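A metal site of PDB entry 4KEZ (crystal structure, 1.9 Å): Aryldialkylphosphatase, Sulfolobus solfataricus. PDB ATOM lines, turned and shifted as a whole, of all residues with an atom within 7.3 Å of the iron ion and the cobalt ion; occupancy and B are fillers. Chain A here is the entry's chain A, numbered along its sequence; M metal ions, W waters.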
ATOM      1  N   HIS A  22     -18.919 -31.182   4.245  1.00  0.00           N
ATOM      2  CA  HIS A  22     -19.065 -29.851   4.826  1.00  0.00           C
ATOM      3  C   HIS A  22     -18.592 -29.825   6.263  1.00  0.00           C
ATOM      4  O   HIS A  22     -19.369 -30.072   7.174  1.00  0.00           O
ATOM      5  CB  HIS A  22     -20.517 -29.385   4.727  1.00  0.00           C
ATOM      6  CG  HIS A  22     -20.722 -27.911   5.001  1.00  0.00           C
ATOM      7  ND1 HIS A  22     -21.455 -27.119   4.187  1.00  0.00           N
ATOM      8  CD2 HIS A  22     -20.255 -27.090   6.035  1.00  0.00           C
ATOM      9  CE1 HIS A  22     -21.462 -25.856   4.670  1.00  0.00           C
ATOM     10  NE2 HIS A  22     -20.733 -25.838   5.796  1.00  0.00           N
ATOM     11  N   GLU A  23     -17.295 -29.540   6.460  1.00  0.00           N
ATOM     12  CA  GLU A  23     -16.734 -29.383   7.811  1.00  0.00           C
ATOM     13  C   GLU A  23     -15.750 -28.201   7.813  1.00  0.00           C
ATOM     14  O   GLU A  23     -15.210 -27.858   6.769  1.00  0.00           O
ATOM     15  CB  GLU A  23     -16.004 -30.654   8.263  1.00  0.00           C
ATOM     16  CG  GLU A  23     -16.738 -31.972   8.048  1.00  0.00           C
ATOM     17  CD  GLU A  23     -17.936 -32.157   8.955  1.00  0.00           C
ATOM     18  OE1 GLU A  23     -18.795 -33.015   8.627  1.00  0.00           O
ATOM     19  OE2 GLU A  23     -18.025 -31.470   9.985  1.00  0.00           O
ATOM     20  N   HIS A  24     -15.530 -27.593   8.975  1.00  0.00           N
ATOM     21  CA  HIS A  24     -14.628 -26.437   9.064  1.00  0.00           C
ATOM     22  C   HIS A  24     -13.481 -26.710  10.017  1.00  0.00           C
ATOM     23  O   HIS A  24     -13.699 -26.988  11.186  1.00  0.00           O
ATOM     24  CB  HIS A  24     -15.360 -25.187   9.562  1.00  0.00           C
ATOM     25  CG  HIS A  24     -16.491 -24.731   8.653  1.00  0.00           C
ATOM     26  ND1 HIS A  24     -16.298 -23.927   7.589  1.00  0.00           N
ATOM     27  CD2 HIS A  24     -17.863 -24.974   8.721  1.00  0.00           C
ATOM     28  CE1 HIS A  24     -17.476 -23.684   6.989  1.00  0.00           C
ATOM     29  NE2 HIS A  24     -18.436 -24.318   7.690  1.00  0.00           N
ATOM     30  N   VAL A  27     -13.047 -21.407  12.004  1.00  0.00           N
ATOM     31  CA  VAL A  27     -13.802 -20.254  11.537  1.00  0.00           C
ATOM     32  C   VAL A  27     -13.470 -19.033  12.394  1.00  0.00           C
ATOM     33  O   VAL A  27     -13.394 -19.129  13.616  1.00  0.00           O
ATOM     34  CB  VAL A  27     -15.327 -20.529  11.589  1.00  0.00           C
ATOM     35  CG1 VAL A  27     -16.129 -19.259  11.345  1.00  0.00           C
ATOM     36  CG2 VAL A  27     -15.711 -21.602  10.580  1.00  0.00           C
ATOM     37  N   ASP A  66     -13.885 -28.396   2.950  1.00  0.00           N
ATOM     38  CA  ASP A  66     -13.975 -27.348   3.959  1.00  0.00           C
ATOM     39  C   ASP A  66     -14.386 -26.036   3.306  1.00  0.00           C
ATOM     40  O   ASP A  66     -13.593 -25.408   2.610  1.00  0.00           O
ATOM     41  CB  ASP A  66     -12.611 -27.193   4.663  1.00  0.00           C
ATOM     42  CG  ASP A  66     -12.619 -26.133   5.754  1.00  0.00           C
ATOM     43  OD1 ASP A  66     -13.511 -25.251   5.760  1.00  0.00           O
ATOM     44  OD2 ASP A  66     -11.708 -26.173   6.615  1.00  0.00           O
ATOM     45  N   PRO A  67     -15.661 -25.638   3.494  1.00  0.00           N
ATOM     46  CA  PRO A  67     -16.169 -24.461   2.800  1.00  0.00           C
ATOM     47  C   PRO A  67     -15.954 -23.143   3.558  1.00  0.00           C
ATOM     48  O   PRO A  67     -16.781 -22.218   3.469  1.00  0.00           O
ATOM     49  CB  PRO A  67     -17.666 -24.752   2.677  1.00  0.00           C
ATOM     50  CG  PRO A  67     -17.982 -25.610   3.854  1.00  0.00           C
ATOM     51  CD  PRO A  67     -16.729 -26.393   4.167  1.00  0.00           C
ATOM     52  N   THR A  68     -14.842 -23.060   4.290  1.00  0.00           N
ATOM     53  CA  THR A  68     -14.412 -21.793   4.890  1.00  0.00           C
ATOM     54  C   THR A  68     -13.873 -20.887   3.783  1.00  0.00           C
ATOM     55  O   THR A  68     -12.868 -21.212   3.133  1.00  0.00           O
ATOM     56  CB  THR A  68     -13.289 -22.037   5.926  1.00  0.00           C
ATOM     57  OG1 THR A  68     -13.696 -23.070   6.829  1.00  0.00           O
ATOM     58  CG2 THR A  68     -12.996 -20.769   6.710  1.00  0.00           C
ATOM     59  N   LEU A  72     -15.493 -16.147   6.620  1.00  0.00           N
ATOM     60  CA  LEU A  72     -15.378 -17.194   7.631  1.00  0.00           C
ATOM     61  C   LEU A  72     -13.925 -17.434   8.041  1.00  0.00           C
ATOM     62  O   LEU A  72     -13.641 -18.334   8.836  1.00  0.00           O
ATOM     63  CB  LEU A  72     -15.982 -18.509   7.133  1.00  0.00           C
ATOM     64  CG  LEU A  72     -17.486 -18.583   6.882  1.00  0.00           C
ATOM     65  CD1 LEU A  72     -17.865 -19.965   6.376  1.00  0.00           C
ATOM     66  CD2 LEU A  72     -18.241 -18.253   8.170  1.00  0.00           C
ATOM     67  N   TYR A  97     -18.918 -15.377   1.759  1.00  0.00           N
ATOM     68  CA  TYR A  97     -19.944 -15.729   2.711  1.00  0.00           C
ATOM     69  C   TYR A  97     -20.450 -14.433   3.342  1.00  0.00           C
ATOM     70  O   TYR A  97     -19.778 -13.849   4.197  1.00  0.00           O
ATOM     71  CB  TYR A  97     -19.354 -16.678   3.758  1.00  0.00           C
ATOM     72  CG  TYR A  97     -20.312 -17.225   4.820  1.00  0.00           C
ATOM     73  CD1 TYR A  97     -20.702 -16.445   5.889  1.00  0.00           C
ATOM     74  CD2 TYR A  97     -20.768 -18.537   4.763  1.00  0.00           C
ATOM     75  CE1 TYR A  97     -21.556 -16.942   6.879  1.00  0.00           C
ATOM     76  CE2 TYR A  97     -21.624 -19.043   5.739  1.00  0.00           C
ATOM     77  CZ  TYR A  97     -22.007 -18.245   6.794  1.00  0.00           C
ATOM     78  OH  TYR A  97     -22.843 -18.737   7.772  1.00  0.00           O
ATOM     79  N   TYR A  99     -24.425 -12.331   4.479  1.00  0.00           N
ATOM     80  CA  TYR A  99     -25.869 -12.457   4.685  1.00  0.00           C
ATOM     81  C   TYR A  99     -26.607 -11.224   4.147  1.00  0.00           C
ATOM     82  O   TYR A  99     -27.776 -11.306   3.774  1.00  0.00           O
ATOM     83  CB  TYR A  99     -26.196 -12.587   6.167  1.00  0.00           C
ATOM     84  CG  TYR A  99     -25.845 -13.921   6.823  1.00  0.00           C
ATOM     85  CD1 TYR A  99     -25.163 -14.916   6.139  1.00  0.00           C
ATOM     86  CD2 TYR A  99     -26.182 -14.150   8.149  1.00  0.00           C
ATOM     87  CE1 TYR A  99     -24.848 -16.120   6.758  1.00  0.00           C
ATOM     88  CE2 TYR A  99     -25.870 -15.342   8.775  1.00  0.00           C
ATOM     89  CZ  TYR A  99     -25.198 -16.324   8.076  1.00  0.00           C
ATOM     90  OH  TYR A  99     -24.884 -17.506   8.716  1.00  0.00           O
ATOM     91  N   KCX A 137     -18.205 -21.363  -2.762  1.00  0.00           N
ATOM     92  CA  KCX A 137     -19.168 -21.359  -1.657  1.00  0.00           C
ATOM     93  CB  KCX A 137     -18.410 -21.567  -0.345  1.00  0.00           C
ATOM     94  CG  KCX A 137     -19.270 -21.230   0.873  1.00  0.00           C
ATOM     95  CD  KCX A 137     -20.304 -22.316   1.144  1.00  0.00           C
ATOM     96  CE  KCX A 137     -21.066 -22.026   2.453  1.00  0.00           C
ATOM     97  NZ  KCX A 137     -20.253 -22.272   3.640  1.00  0.00           N
ATOM     98  C   KCX A 137     -19.876 -20.032  -1.626  1.00  0.00           C
ATOM     99  O   KCX A 137     -19.243 -18.990  -1.736  1.00  0.00           O
ATOM    100  CX  KCX A 137     -20.801 -22.636   4.805  1.00  0.00           C
ATOM    101  OQ1 KCX A 137     -20.010 -22.839   5.850  1.00  0.00           O
ATOM    102  OQ2 KCX A 137     -22.002 -22.804   4.968  1.00  0.00           O
ATOM    103  N   ILE A 138     -21.196 -20.073  -1.498  1.00  0.00           N
ATOM    104  CA  ILE A 138     -22.006 -18.851  -1.373  1.00  0.00           C
ATOM    105  C   ILE A 138     -23.029 -19.059  -0.258  1.00  0.00           C
ATOM    106  O   ILE A 138     -23.283 -20.187   0.165  1.00  0.00           O
ATOM    107  CB  ILE A 138     -22.707 -18.503  -2.703  1.00  0.00           C
ATOM    108  CG1 ILE A 138     -23.723 -19.581  -3.076  1.00  0.00           C
ATOM    109  CG2 ILE A 138     -21.701 -18.321  -3.827  1.00  0.00           C
ATOM    110  CD1 ILE A 138     -25.091 -19.394  -2.433  1.00  0.00           C
ATOM    111  N   ALA A 139     -23.609 -17.956   0.227  1.00  0.00           N
ATOM    112  CA  ALA A 139     -24.533 -18.029   1.355  1.00  0.00           C
ATOM    113  C   ALA A 139     -25.735 -17.110   1.230  1.00  0.00           C
ATOM    114  O   ALA A 139     -25.703 -16.110   0.510  1.00  0.00           O
ATOM    115  CB  ALA A 139     -23.793 -17.712   2.660  1.00  0.00           C
ATOM    116  N   ASP A 141     -29.120 -16.198   4.291  1.00  0.00           N
ATOM    117  CA  ASP A 141     -29.715 -16.664   5.530  1.00  0.00           C
ATOM    118  C   ASP A 141     -30.996 -15.884   5.803  1.00  0.00           C
ATOM    119  O   ASP A 141     -31.765 -15.596   4.887  1.00  0.00           O
ATOM    120  CB  ASP A 141     -28.702 -16.555   6.688  1.00  0.00           C
ATOM    121  CG  ASP A 141     -28.998 -17.536   7.823  1.00  0.00           C
ATOM    122  OD1 ASP A 141     -29.971 -17.319   8.574  1.00  0.00           O
ATOM    123  OD2 ASP A 141     -28.233 -18.516   7.987  1.00  0.00           O
ATOM    124  N   THR A 169     -23.644 -24.323  -1.101  1.00  0.00           N
ATOM    125  CA  THR A 169     -24.304 -23.174  -0.508  1.00  0.00           C
ATOM    126  C   THR A 169     -24.581 -23.332   0.977  1.00  0.00           C
ATOM    127  O   THR A 169     -24.640 -24.446   1.496  1.00  0.00           O
ATOM    128  CB  THR A 169     -25.627 -22.825  -1.209  1.00  0.00           C
ATOM    129  OG1 THR A 169     -26.691 -23.610  -0.656  1.00  0.00           O
ATOM    130  CG2 THR A 169     -25.531 -23.080  -2.712  1.00  0.00           C
ATOM    131  N   HIS A 170     -24.720 -22.186   1.615  1.00  0.00           N
ATOM    132  CA  HIS A 170     -25.266 -22.046   2.950  1.00  0.00           C
ATOM    133  C   HIS A 170     -26.615 -21.454   2.737  1.00  0.00           C
ATOM    134  O   HIS A 170     -26.753 -20.469   2.008  1.00  0.00           O
ATOM    135  CB  HIS A 170     -24.411 -21.058   3.738  1.00  0.00           C
ATOM    136  CG  HIS A 170     -24.985 -20.675   5.079  1.00  0.00           C
ATOM    137  ND1 HIS A 170     -24.471 -21.113   6.242  1.00  0.00           N
ATOM    138  CD2 HIS A 170     -26.054 -19.834   5.422  1.00  0.00           C
ATOM    139  CE1 HIS A 170     -25.175 -20.594   7.278  1.00  0.00           C
ATOM    140  NE2 HIS A 170     -26.149 -19.819   6.769  1.00  0.00           N
ATOM    141  N   SER A 171     -27.640 -22.053   3.342  1.00  0.00           N
ATOM    142  CA  SER A 171     -28.974 -21.460   3.279  1.00  0.00           C
ATOM    143  C   SER A 171     -29.654 -21.549   4.641  1.00  0.00           C
ATOM    144  O   SER A 171     -29.138 -22.194   5.563  1.00  0.00           O
ATOM    145  CB  SER A 171     -29.840 -22.119   2.200  1.00  0.00           C
ATOM    146  OG  SER A 171     -30.464 -23.310   2.672  1.00  0.00           O
ATOM    147  N   GLY A 198     -27.283 -26.138   0.900  1.00  0.00           N
ATOM    148  CA  GLY A 198     -26.857 -26.475   2.249  1.00  0.00           C
ATOM    149  C   GLY A 198     -27.884 -26.247   3.343  1.00  0.00           C
ATOM    150  O   GLY A 198     -28.771 -25.416   3.222  1.00  0.00           O
ATOM    151  N   HIS A 199     -27.740 -27.030   4.413  1.00  0.00           N
ATOM    152  CA  HIS A 199     -28.479 -26.832   5.673  1.00  0.00           C
ATOM    153  C   HIS A 199     -29.932 -27.161   5.595  1.00  0.00           C
ATOM    154  O   HIS A 199     -30.732 -26.731   6.441  1.00  0.00           O
ATOM    155  CB  HIS A 199     -28.210 -25.434   6.237  1.00  0.00           C
ATOM    156  CG  HIS A 199     -26.745 -25.077   6.288  1.00  0.00           C
ATOM    157  ND1 HIS A 199     -25.783 -26.009   6.449  1.00  0.00           N
ATOM    158  CD2 HIS A 199     -26.086 -23.853   6.186  1.00  0.00           C
ATOM    159  CE1 HIS A 199     -24.571 -25.415   6.464  1.00  0.00           C
ATOM    160  NE2 HIS A 199     -24.760 -24.096   6.299  1.00  0.00           N
ATOM    161  N   ASP A 222     -26.664 -31.627   6.645  1.00  0.00           N
ATOM    162  CA  ASP A 222     -25.241 -31.386   6.842  1.00  0.00           C
ATOM    163  C   ASP A 222     -24.874 -30.717   8.167  1.00  0.00           C
ATOM    164  O   ASP A 222     -23.769 -30.215   8.311  1.00  0.00           O
ATOM    165  CB  ASP A 222     -24.726 -30.534   5.697  1.00  0.00           C
ATOM    166  CG  ASP A 222     -25.490 -29.227   5.541  1.00  0.00           C
ATOM    167  OD1 ASP A 222     -26.176 -28.797   6.507  1.00  0.00           O
ATOM    168  OD2 ASP A 222     -25.418 -28.624   4.448  1.00  0.00           O
ATOM    169  N   ARG A 223     -25.792 -30.715   9.126  1.00  0.00           N
ATOM    170  CA  ARG A 223     -25.515 -30.076  10.411  1.00  0.00           C
ATOM    171  C   ARG A 223     -25.792 -30.991  11.605  1.00  0.00           C
ATOM    172  O   ARG A 223     -26.234 -30.553  12.678  1.00  0.00           O
ATOM    173  CB  ARG A 223     -26.262 -28.738  10.532  1.00  0.00           C
ATOM    174  CG  ARG A 223     -25.568 -27.608   9.781  1.00  0.00           C
ATOM    175  CD  ARG A 223     -26.386 -26.317   9.813  1.00  0.00           C
ATOM    176  NE  ARG A 223     -25.533 -25.121   9.808  1.00  0.00           N
ATOM    177  CZ  ARG A 223     -26.006 -23.885   9.775  1.00  0.00           C
ATOM    178  NH1 ARG A 223     -27.316 -23.671   9.720  1.00  0.00           N
ATOM    179  NH2 ARG A 223     -25.177 -22.840   9.797  1.00  0.00           N
ATOM    180  N   HIS A 255     -21.560 -32.617   9.287  1.00  0.00           N
ATOM    181  CA  HIS A 255     -21.819 -32.025  10.604  1.00  0.00           C
ATOM    182  C   HIS A 255     -21.720 -30.535  10.626  1.00  0.00           C
ATOM    183  O   HIS A 255     -22.240 -29.897  11.546  1.00  0.00           O
ATOM    184  CB  HIS A 255     -20.837 -32.539  11.646  1.00  0.00           C
ATOM    185  CG  HIS A 255     -20.647 -34.035  11.634  1.00  0.00           C
ATOM    186  ND1 HIS A 255     -19.699 -34.645  10.888  1.00  0.00           N
ATOM    187  CD2 HIS A 255     -21.295 -35.042  12.345  1.00  0.00           C
ATOM    188  CE1 HIS A 255     -19.750 -35.978  11.103  1.00  0.00           C
ATOM    189  NE2 HIS A 255     -20.732 -36.216  11.987  1.00  0.00           N
ATOM    190  N   ASP A 256     -21.033 -29.959   9.640  1.00  0.00           N
ATOM    191  CA  ASP A 256     -20.726 -28.520   9.660  1.00  0.00           C
ATOM    192  C   ASP A 256     -19.898 -28.221  10.899  1.00  0.00           C
ATOM    193  O   ASP A 256     -19.970 -27.128  11.477  1.00  0.00           O
ATOM    194  CB  ASP A 256     -22.026 -27.686   9.684  1.00  0.00           C
ATOM    195  CG  ASP A 256     -21.799 -26.221   9.296  1.00  0.00           C
ATOM    196  OD1 ASP A 256     -20.730 -25.893   8.757  1.00  0.00           O
ATOM    197  OD2 ASP A 256     -22.723 -25.395   9.512  1.00  0.00           O
ATOM    198  N   TYR A 257     -19.118 -29.201  11.333  1.00  0.00           N
ATOM    199  CA  TYR A 257     -18.404 -29.033  12.586  1.00  0.00           C
ATOM    200  C   TYR A 257     -17.283 -28.012  12.477  1.00  0.00           C
ATOM    201  O   TYR A 257     -16.493 -28.034  11.524  1.00  0.00           O
ATOM    202  CB  TYR A 257     -17.863 -30.356  13.126  1.00  0.00           C
ATOM    203  CG  TYR A 257     -17.318 -30.174  14.526  1.00  0.00           C
ATOM    204  CD1 TYR A 257     -18.183 -29.917  15.587  1.00  0.00           C
ATOM    205  CD2 TYR A 257     -15.954 -30.220  14.776  1.00  0.00           C
ATOM    206  CE1 TYR A 257     -17.688 -29.725  16.870  1.00  0.00           C
ATOM    207  CE2 TYR A 257     -15.458 -30.029  16.044  1.00  0.00           C
ATOM    208  CZ  TYR A 257     -16.325 -29.781  17.092  1.00  0.00           C
ATOM    209  OH  TYR A 257     -15.822 -29.592  18.354  1.00  0.00           O
ATOM    210  N   CYS A 258     -17.214 -27.115  13.452  1.00  0.00           N
ATOM    211  CA  CYS A 258     -16.136 -26.147  13.510  1.00  0.00           C
ATOM    212  C   CYS A 258     -15.172 -26.507  14.642  1.00  0.00           C
ATOM    213  O   CYS A 258     -15.535 -26.406  15.811  1.00  0.00           O
ATOM    214  CB  CYS A 258     -16.697 -24.737  13.712  1.00  0.00           C
ATOM    215  SG  CYS A 258     -17.891 -24.241  12.453  1.00  0.00           S
HETATM  216 FE    FE M   1     -20.397 -24.322   7.199  1.00  0.00          FE
HETATM  217 CO    CO M   2     -23.253 -22.770   6.432  1.00  0.00          CO
HETATM  218  O   HOH W   1     -21.894 -21.120   9.113  1.00  0.00           O
HETATM  219  O   HOH W   2     -22.007 -23.469   7.878  1.00  0.00           O
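Along chain A the residues within 4 Å of the iron ion span positions 22 to 256. The nearest printed residue that does not touch the iron ion is Pro 67 (4.3 Å).
Merely in contact with the cobalt ion: Arg 223 (3.9 Å). Within 4 Å of the cobalt ion: His 22, KCX 137, His 170, His 199 and Arg 223. The nearest printed residue that does not touch the cobalt ion is Asp 256 (4.1 Å).
The iron ion is bound by water W2 (1.9 Å), a ring nitrogen (NE2) of His 24 (2.0 Å), OQ1 of KCX 137 (2.0 Å), a ring nitrogen (NE2) of His 22 (2.1 Å) and the side-chain carboxylate of Asp 256 (2.2 Å).
NE of Arg 223 lies close to ND1 of His 199 (3.5 Å). The side-chain hydroxyl of Thr 68 lies within hydrogen-bond range of a ring nitrogen (ND1) of His 24 (2.8 Å). N of His 24 sits at hydrogen-bond distance from O of Tyr 257 (2.8 Å). A ring nitrogen (NE2) of His 170 lies within hydrogen-bond range of the side-chain hydroxyl of Tyr 99. N of His 170 lies within hydrogen-bond range of O of Ile 138 (2.9 Å). The side-chain carboxylate of Asp 256 lies within salt-bridge range of the guanidinium group of Arg 223 (2.8 Å). The backbone NH (N) of Asp 256 lies within hydrogen-bond range of the side-chain carboxylate (OE2) of Glu 23, at 3.4 Å. The backbone NH (N) of Asp 256 is in hydrogen-bond range of the backbone carbonyl oxygen (O) of Asp 222, 3.1 Å away.
The cobalt ion is bound by OQ2 of KCX 137. NE2 of His 199 is bound to the cobalt ion, at 2.0 Å. Water W2 binds the cobalt ion (2.0 Å). A ring nitrogen (ND1) of His 170 binds the cobalt ion (2.1 Å). The cobalt ion has four donor atoms within binding distance.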
